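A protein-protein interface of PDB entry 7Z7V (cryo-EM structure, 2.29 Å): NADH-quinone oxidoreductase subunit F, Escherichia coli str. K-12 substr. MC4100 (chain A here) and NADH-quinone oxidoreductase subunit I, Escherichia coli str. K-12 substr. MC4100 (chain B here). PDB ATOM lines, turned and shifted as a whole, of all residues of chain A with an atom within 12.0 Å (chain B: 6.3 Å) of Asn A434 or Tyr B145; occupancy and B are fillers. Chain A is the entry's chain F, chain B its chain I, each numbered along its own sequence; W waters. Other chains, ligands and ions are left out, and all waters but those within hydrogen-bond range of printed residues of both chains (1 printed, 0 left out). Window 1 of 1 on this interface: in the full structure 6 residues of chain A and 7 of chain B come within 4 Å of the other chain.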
ATOM      1  N   THR A 430      -5.349  15.737  12.464  1.00  0.00           N
ATOM      2  CA  THR A 430      -5.559  14.706  13.464  1.00  0.00           C
ATOM      3  C   THR A 430      -5.156  13.348  12.910  1.00  0.00           C
ATOM      4  O   THR A 430      -5.059  13.150  11.697  1.00  0.00           O
ATOM      5  CB  THR A 430      -7.030  14.643  13.902  1.00  0.00           C
ATOM      6  OG1 THR A 430      -7.824  14.125  12.827  1.00  0.00           O
ATOM      7  CG2 THR A 430      -7.551  16.005  14.274  1.00  0.00           C
ATOM      8  N   HIS A 431      -4.924  12.408  13.818  1.00  0.00           N
ATOM      9  CA  HIS A 431      -4.855  11.001  13.468  1.00  0.00           C
ATOM     10  C   HIS A 431      -5.998  10.269  14.154  1.00  0.00           C
ATOM     11  O   HIS A 431      -6.600  10.770  15.106  1.00  0.00           O
ATOM     12  CB  HIS A 431      -3.507  10.372  13.846  1.00  0.00           C
ATOM     13  CG  HIS A 431      -3.137  10.536  15.285  1.00  0.00           C
ATOM     14  ND1 HIS A 431      -3.686   9.769  16.289  1.00  0.00           N
ATOM     15  CD2 HIS A 431      -2.253  11.365  15.887  1.00  0.00           C
ATOM     16  CE1 HIS A 431      -3.167  10.128  17.448  1.00  0.00           C
ATOM     17  NE2 HIS A 431      -2.295  11.095  17.232  1.00  0.00           N
ATOM     18  N   LEU A 432      -6.311   9.087  13.643  1.00  0.00           N
ATOM     19  CA  LEU A 432      -7.388   8.296  14.214  1.00  0.00           C
ATOM     20  C   LEU A 432      -6.966   7.712  15.553  1.00  0.00           C
ATOM     21  O   LEU A 432      -5.826   7.277  15.729  1.00  0.00           O
ATOM     22  CB  LEU A 432      -7.790   7.176  13.258  1.00  0.00           C
ATOM     23  CG  LEU A 432      -8.554   7.599  12.004  1.00  0.00           C
ATOM     24  CD1 LEU A 432      -9.021   6.377  11.245  1.00  0.00           C
ATOM     25  CD2 LEU A 432      -9.731   8.492  12.362  1.00  0.00           C
ATOM     26  N   ILE A 433      -7.889   7.721  16.505  1.00  0.00           N
ATOM     27  CA  ILE A 433      -7.702   7.067  17.792  1.00  0.00           C
ATOM     28  C   ILE A 433      -8.689   5.917  17.856  1.00  0.00           C
ATOM     29  O   ILE A 433      -9.903   6.125  17.742  1.00  0.00           O
ATOM     30  CB  ILE A 433      -7.897   8.041  18.963  1.00  0.00           C
ATOM     31  CG1 ILE A 433      -6.807   9.113  18.943  1.00  0.00           C
ATOM     32  CG2 ILE A 433      -7.882   7.293  20.285  1.00  0.00           C
ATOM     33  CD1 ILE A 433      -7.183  10.369  19.663  1.00  0.00           C
ATOM     34  N   ASN A 434      -8.169   4.706  18.026  1.00  0.00           N
ATOM     35  CA  ASN A 434      -9.002   3.513  17.999  1.00  0.00           C
ATOM     36  C   ASN A 434      -9.934   3.481  19.202  1.00  0.00           C
ATOM     37  O   ASN A 434      -9.489   3.577  20.349  1.00  0.00           O
ATOM     38  CB  ASN A 434      -8.124   2.263  17.972  1.00  0.00           C
ATOM     39  CG  ASN A 434      -8.833   1.067  17.383  1.00  0.00           C
ATOM     40  OD1 ASN A 434     -10.031   1.113  17.110  1.00  0.00           O
ATOM     41  ND2 ASN A 434      -8.095  -0.018  17.185  1.00  0.00           N
ATOM     42  N   GLY A 435     -11.228   3.346  18.936  1.00  0.00           N
ATOM     43  CA  GLY A 435     -12.237   3.338  19.969  1.00  0.00           C
ATOM     44  C   GLY A 435     -13.019   4.626  20.109  1.00  0.00           C
ATOM     45  O   GLY A 435     -14.055   4.628  20.780  1.00  0.00           O
ATOM     46  N   ILE A 436     -12.566   5.713  19.495  1.00  0.00           N
ATOM     47  CA  ILE A 436     -13.245   7.000  19.575  1.00  0.00           C
ATOM     48  C   ILE A 436     -13.689   7.391  18.175  1.00  0.00           C
ATOM     49  O   ILE A 436     -12.857   7.550  17.275  1.00  0.00           O
ATOM     50  CB  ILE A 436     -12.345   8.083  20.189  1.00  0.00           C
ATOM     51  CG1 ILE A 436     -11.959   7.696  21.613  1.00  0.00           C
ATOM     52  CG2 ILE A 436     -13.051   9.422  20.188  1.00  0.00           C
ATOM     53  CD1 ILE A 436     -10.869   8.532  22.191  1.00  0.00           C
ATOM     54  N   GLN A 437     -14.990   7.543  17.993  1.00  0.00           N
ATOM     55  CA  GLN A 437     -15.521   7.986  16.711  1.00  0.00           C
ATOM     56  C   GLN A 437     -15.358   9.495  16.580  1.00  0.00           C
ATOM     57  O   GLN A 437     -15.789  10.237  17.466  1.00  0.00           O
ATOM     58  CB  GLN A 437     -16.985   7.604  16.573  1.00  0.00           C
ATOM     59  CG  GLN A 437     -17.213   6.165  16.173  1.00  0.00           C
ATOM     60  CD  GLN A 437     -18.615   5.700  16.481  1.00  0.00           C
ATOM     61  OE1 GLN A 437     -18.980   5.528  17.640  1.00  0.00           O
ATOM     62  NE2 GLN A 437     -19.413   5.500  15.443  1.00  0.00           N
ATOM     63  N   PRO A 438     -14.743   9.981  15.508  1.00  0.00           N
ATOM     64  CA  PRO A 438     -14.489  11.418  15.389  1.00  0.00           C
ATOM     65  C   PRO A 438     -15.757  12.210  15.102  1.00  0.00           C
ATOM     66  O   PRO A 438     -16.749  11.695  14.585  1.00  0.00           O
ATOM     67  CB  PRO A 438     -13.504  11.507  14.220  1.00  0.00           C
ATOM     68  CG  PRO A 438     -13.806  10.313  13.401  1.00  0.00           C
ATOM     69  CD  PRO A 438     -14.222   9.231  14.354  1.00  0.00           C
ATOM     70  N   ASN A 439     -15.704  13.490  15.457  1.00  0.00           N
ATOM     71  CA  ASN A 439     -16.780  14.437  15.179  1.00  0.00           C
ATOM     72  C   ASN A 439     -16.539  15.018  13.793  1.00  0.00           C
ATOM     73  O   ASN A 439     -15.680  15.882  13.611  1.00  0.00           O
ATOM     74  CB  ASN A 439     -16.827  15.523  16.247  1.00  0.00           C
ATOM     75  CG  ASN A 439     -18.124  16.295  16.237  1.00  0.00           C
ATOM     76  OD1 ASN A 439     -19.203  15.713  16.246  1.00  0.00           O
ATOM     77  ND2 ASN A 439     -18.025  17.614  16.227  1.00  0.00           N
ATOM     78  N   THR B  51      -6.775   1.276  33.235  1.00  0.00           N
ATOM     79  CA  THR B  51      -6.153   0.500  32.175  1.00  0.00           C
ATOM     80  C   THR B  51      -4.684   0.869  32.010  1.00  0.00           C
ATOM     81  O   THR B  51      -4.171   1.801  32.630  1.00  0.00           O
ATOM     82  CB  THR B  51      -6.903   0.695  30.855  1.00  0.00           C
ATOM     83  OG1 THR B  51      -6.910   2.082  30.507  1.00  0.00           O
ATOM     84  CG2 THR B  51      -8.330   0.210  30.991  1.00  0.00           C
ATOM     85  N   ARG B  52      -4.013   0.112  31.151  1.00  0.00           N
ATOM     86  CA  ARG B  52      -2.592   0.260  30.896  1.00  0.00           C
ATOM     87  C   ARG B  52      -2.359   0.681  29.453  1.00  0.00           C
ATOM     88  O   ARG B  52      -3.189   0.448  28.576  1.00  0.00           O
ATOM     89  CB  ARG B  52      -1.840  -1.041  31.184  1.00  0.00           C
ATOM     90  CG  ARG B  52      -1.830  -1.427  32.642  1.00  0.00           C
ATOM     91  CD  ARG B  52      -1.096  -2.726  32.867  1.00  0.00           C
ATOM     92  NE  ARG B  52      -1.177  -3.145  34.259  1.00  0.00           N
ATOM     93  CZ  ARG B  52      -0.310  -2.794  35.197  1.00  0.00           C
ATOM     94  NH1 ARG B  52       0.725  -2.016  34.926  1.00  0.00           N
ATOM     95  NH2 ARG B  52      -0.485  -3.231  36.438  1.00  0.00           N
ATOM     96  N   PRO B  54      -0.179   0.560  25.784  1.00  0.00           N
ATOM     97  CA  PRO B  54       0.412  -0.572  25.047  1.00  0.00           C
ATOM     98  C   PRO B  54       1.805  -0.970  25.514  1.00  0.00           C
ATOM     99  O   PRO B  54       2.193  -2.127  25.325  1.00  0.00           O
ATOM    100  CB  PRO B  54       0.436  -0.069  23.599  1.00  0.00           C
ATOM    101  CG  PRO B  54      -0.701   0.856  23.520  1.00  0.00           C
ATOM    102  CD  PRO B  54      -0.819   1.519  24.860  1.00  0.00           C
ATOM    103  N   ARG B  59      -1.966   3.856  32.634  1.00  0.00           N
ATOM    104  CA  ARG B  59      -2.233   5.077  31.890  1.00  0.00           C
ATOM    105  C   ARG B  59      -2.516   6.267  32.791  1.00  0.00           C
ATOM    106  O   ARG B  59      -2.366   7.406  32.342  1.00  0.00           O
ATOM    107  CB  ARG B  59      -3.410   4.869  30.941  1.00  0.00           C
ATOM    108  CG  ARG B  59      -3.070   4.052  29.732  1.00  0.00           C
ATOM    109  CD  ARG B  59      -3.926   4.406  28.547  1.00  0.00           C
ATOM    110  NE  ARG B  59      -5.050   3.499  28.389  1.00  0.00           N
ATOM    111  CZ  ARG B  59      -5.380   2.911  27.251  1.00  0.00           C
ATOM    112  NH1 ARG B  59      -4.681   3.101  26.146  1.00  0.00           N
ATOM    113  NH2 ARG B  59      -6.444   2.120  27.219  1.00  0.00           N
ATOM    114  N   GLU B 106     -15.022   8.616  32.815  1.00  0.00           N
ATOM    115  CA  GLU B 106     -14.400   8.132  31.586  1.00  0.00           C
ATOM    116  C   GLU B 106     -14.416   9.206  30.509  1.00  0.00           C
ATOM    117  O   GLU B 106     -13.446   9.359  29.759  1.00  0.00           O
ATOM    118  CB  GLU B 106     -15.105   6.866  31.094  1.00  0.00           C
ATOM    119  CG  GLU B 106     -14.610   6.375  29.737  1.00  0.00           C
ATOM    120  CD  GLU B 106     -15.298   5.117  29.256  1.00  0.00           C
ATOM    121  OE1 GLU B 106     -15.815   4.351  30.091  1.00  0.00           O
ATOM    122  OE2 GLU B 106     -15.313   4.891  28.030  1.00  0.00           O
ATOM    123  N   THR B 112      -7.506   8.210  28.741  1.00  0.00           N
ATOM    124  CA  THR B 112      -8.315   6.985  28.637  1.00  0.00           C
ATOM    125  C   THR B 112      -7.907   5.929  29.664  1.00  0.00           C
ATOM    126  O   THR B 112      -8.041   4.731  29.415  1.00  0.00           O
ATOM    127  CB  THR B 112      -8.295   6.376  27.226  1.00  0.00           C
ATOM    128  OG1 THR B 112      -7.029   5.754  26.982  1.00  0.00           O
ATOM    129  CG2 THR B 112      -8.552   7.429  26.173  1.00  0.00           C
ATOM    130  N   ILE B 114      -9.249   5.612  32.933  1.00  0.00           N
ATOM    131  CA  ILE B 114     -10.432   5.133  33.631  1.00  0.00           C
ATOM    132  C   ILE B 114     -11.503   4.805  32.596  1.00  0.00           C
ATOM    133  O   ILE B 114     -11.726   5.564  31.647  1.00  0.00           O
ATOM    134  CB  ILE B 114     -10.909   6.157  34.682  1.00  0.00           C
ATOM    135  CG1 ILE B 114     -12.062   5.618  35.502  1.00  0.00           C
ATOM    136  CG2 ILE B 114     -11.305   7.484  34.082  1.00  0.00           C
ATOM    137  CD1 ILE B 114     -12.187   6.266  36.855  1.00  0.00           C
ATOM    138  N   GLN B 115     -12.103   3.626  32.726  1.00  0.00           N
ATOM    139  CA  GLN B 115     -13.040   3.133  31.729  1.00  0.00           C
ATOM    140  C   GLN B 115     -14.156   2.368  32.415  1.00  0.00           C
ATOM    141  O   GLN B 115     -13.898   1.539  33.289  1.00  0.00           O
ATOM    142  CB  GLN B 115     -12.346   2.220  30.711  1.00  0.00           C
ATOM    143  CG  GLN B 115     -11.491   2.933  29.685  1.00  0.00           C
ATOM    144  CD  GLN B 115     -10.644   1.978  28.880  1.00  0.00           C
ATOM    145  OE1 GLN B 115     -11.069   0.872  28.571  1.00  0.00           O
ATOM    146  NE2 GLN B 115      -9.439   2.401  28.537  1.00  0.00           N
ATOM    147  N   PRO B 142      -5.165  -2.516  27.796  1.00  0.00           N
ATOM    148  CA  PRO B 142      -5.712  -1.197  27.463  1.00  0.00           C
ATOM    149  C   PRO B 142      -7.226  -1.072  27.489  1.00  0.00           C
ATOM    150  O   PRO B 142      -7.724   0.058  27.402  1.00  0.00           O
ATOM    151  CB  PRO B 142      -5.176  -0.969  26.043  1.00  0.00           C
ATOM    152  CG  PRO B 142      -5.063  -2.323  25.474  1.00  0.00           C
ATOM    153  CD  PRO B 142      -4.740  -3.259  26.598  1.00  0.00           C
ATOM    154  N   GLY B 143      -7.965  -2.168  27.605  1.00  0.00           N
ATOM    155  CA  GLY B 143      -9.413  -2.062  27.684  1.00  0.00           C
ATOM    156  C   GLY B 143     -10.027  -1.674  26.352  1.00  0.00           C
ATOM    157  O   GLY B 143      -9.696  -2.235  25.304  1.00  0.00           O
ATOM    158  N   LYS B 144     -10.931  -0.695  26.389  1.00  0.00           N
ATOM    159  CA  LYS B 144     -11.711  -0.320  25.216  1.00  0.00           C
ATOM    160  C   LYS B 144     -10.933   0.514  24.208  1.00  0.00           C
ATOM    161  O   LYS B 144     -11.347   0.595  23.049  1.00  0.00           O
ATOM    162  CB  LYS B 144     -12.962   0.452  25.642  1.00  0.00           C
ATOM    163  CG  LYS B 144     -13.901  -0.336  26.525  1.00  0.00           C
ATOM    164  CD  LYS B 144     -15.229   0.374  26.687  1.00  0.00           C
ATOM    165  CE  LYS B 144     -15.072   1.651  27.476  1.00  0.00           C
ATOM    166  NZ  LYS B 144     -16.381   2.173  27.946  1.00  0.00           N
ATOM    167  N   TYR B 145      -9.833   1.137  24.614  1.00  0.00           N
ATOM    168  CA  TYR B 145      -9.024   1.970  23.725  1.00  0.00           C
ATOM    169  C   TYR B 145      -7.644   1.348  23.604  1.00  0.00           C
ATOM    170  O   TYR B 145      -6.793   1.538  24.490  1.00  0.00           O
ATOM    171  CB  TYR B 145      -8.940   3.401  24.249  1.00  0.00           C
ATOM    172  CG  TYR B 145     -10.290   3.969  24.599  1.00  0.00           C
ATOM    173  CD1 TYR B 145     -11.140   4.443  23.611  1.00  0.00           C
ATOM    174  CD2 TYR B 145     -10.728   4.009  25.913  1.00  0.00           C
ATOM    175  CE1 TYR B 145     -12.380   4.951  23.924  1.00  0.00           C
ATOM    176  CE2 TYR B 145     -11.964   4.517  26.235  1.00  0.00           C
ATOM    177  CZ  TYR B 145     -12.786   4.988  25.238  1.00  0.00           C
ATOM    178  OH  TYR B 145     -14.021   5.496  25.555  1.00  0.00           O
ATOM    179  N   PRO B 146      -7.369   0.604  22.530  1.00  0.00           N
ATOM    180  CA  PRO B 146      -6.194  -0.275  22.527  1.00  0.00           C
ATOM    181  C   PRO B 146      -4.856   0.414  22.331  1.00  0.00           C
ATOM    182  O   PRO B 146      -3.835  -0.157  22.734  1.00  0.00           O
ATOM    183  CB  PRO B 146      -6.482  -1.235  21.367  1.00  0.00           C
ATOM    184  CG  PRO B 146      -7.363  -0.471  20.465  1.00  0.00           C
ATOM    185  CD  PRO B 146      -8.192   0.437  21.321  1.00  0.00           C
ATOM    186  N   GLU B 147      -4.806   1.607  21.744  1.00  0.00           N
ATOM    187  CA  GLU B 147      -3.535   2.153  21.295  1.00  0.00           C
ATOM    188  C   GLU B 147      -3.170   3.518  21.858  1.00  0.00           C
ATOM    189  O   GLU B 147      -2.024   3.940  21.673  1.00  0.00           O
ATOM    190  CB  GLU B 147      -3.510   2.245  19.762  1.00  0.00           C
ATOM    191  CG  GLU B 147      -3.428   0.904  19.064  1.00  0.00           C
ATOM    192  CD  GLU B 147      -4.232   0.872  17.781  1.00  0.00           C
ATOM    193  OE1 GLU B 147      -4.124   1.830  16.986  1.00  0.00           O
ATOM    194  OE2 GLU B 147      -4.972  -0.109  17.567  1.00  0.00           O
ATOM    195  N   TYR B 148      -4.084   4.224  22.519  1.00  0.00           N
ATOM    196  CA  TYR B 148      -3.785   5.591  22.923  1.00  0.00           C
ATOM    197  C   TYR B 148      -2.772   5.625  24.057  1.00  0.00           C
ATOM    198  O   TYR B 148      -2.866   4.871  25.028  1.00  0.00           O
ATOM    199  CB  TYR B 148      -5.043   6.341  23.351  1.00  0.00           C
ATOM    200  CG  TYR B 148      -4.749   7.797  23.625  1.00  0.00           C
ATOM    201  CD1 TYR B 148      -4.484   8.674  22.584  1.00  0.00           C
ATOM    202  CD2 TYR B 148      -4.690   8.287  24.924  1.00  0.00           C
ATOM    203  CE1 TYR B 148      -4.196   9.999  22.823  1.00  0.00           C
ATOM    204  CE2 TYR B 148      -4.401   9.610  25.172  1.00  0.00           C
ATOM    205  CZ  TYR B 148      -4.156  10.461  24.119  1.00  0.00           C
ATOM    206  OH  TYR B 148      -3.869  11.780  24.359  1.00  0.00           O
HETATM  207  O   HOH W   1      -6.858   3.838  21.079  1.00  0.00           O
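The side-chain carboxylate (OE2) of Glu B106 sits at hydrogen-bond distance from the side-chain hydroxyl (OH) of Tyr B145. The guanidinium group of Arg B59 is in hydrogen-bond range of the backbone carbonyl oxygen of Tyr B145, at 2.8 Å.
Water W1 lies within hydrogen-bond range of O of Asn A434 (2.7 Å), N of Glu B147 (3.1 Å) and N of Tyr B148 (3.1 Å).
Hydrophobic or aromatic side chains of chain A within 4 Å of the printed part of chain B: Ile A436. Of the 15 printed residues of chain B, 3 touch a printed residue of chain A. Hydrophobic or aromatic side chains of chain B that line the printed part of chain A: Tyr B145 and Pro B146. Among the printed residues, 5 pairs touch across the chains. Among the printed residues, no Asp or Glu carboxylate lies within 4 Å of a Lys or Arg side-chain nitrogen of the other chain.
Asn A434 touches three residues of chain B. Of chain A, only Asn A434 (3.8 Å), Gly A435 (3.6 Å) and Ile A436 (3.6 Å) come within 4 Å of Tyr B145. No residue of chain A comes within 4 Å of Gln B115. Pro B142 touches none of the printed residues of chain A. No residue of chain A comes within 4 Å of Lys B144. Pro B146 touches just one residue of chain A: Asn A434 (3.4 Å). Printed residues of chain A within 4 Å of Glu B147: Asn A434 (3.1 Å). Of the printed residues of chain B, Gly A435 touches Tyr B145 (3.6 Å). Printed residues of chain B within 4 Å of Ile A436: Tyr B145. Gln A437 touches none of the printed residues of chain B. Ile B114 touches none of the printed residues of chain A. The nearest residue of chain B that does not touch Asn A434 is Lys B144 (4.4 Å). The nearest printed residue of chain B that does not touch Ile A436 is Thr B112 (4.7 Å).
ND2 of Asn A434 sits at hydrogen-bond distance from OE2 of Glu B147 (3.1 Å).
Among the printed residues, merely in contact across the chains: Asn A434 with Tyr B145, Asn A434 with Pro B146, Gly A435 with Tyr B145 and Ile A436 with Tyr B145.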
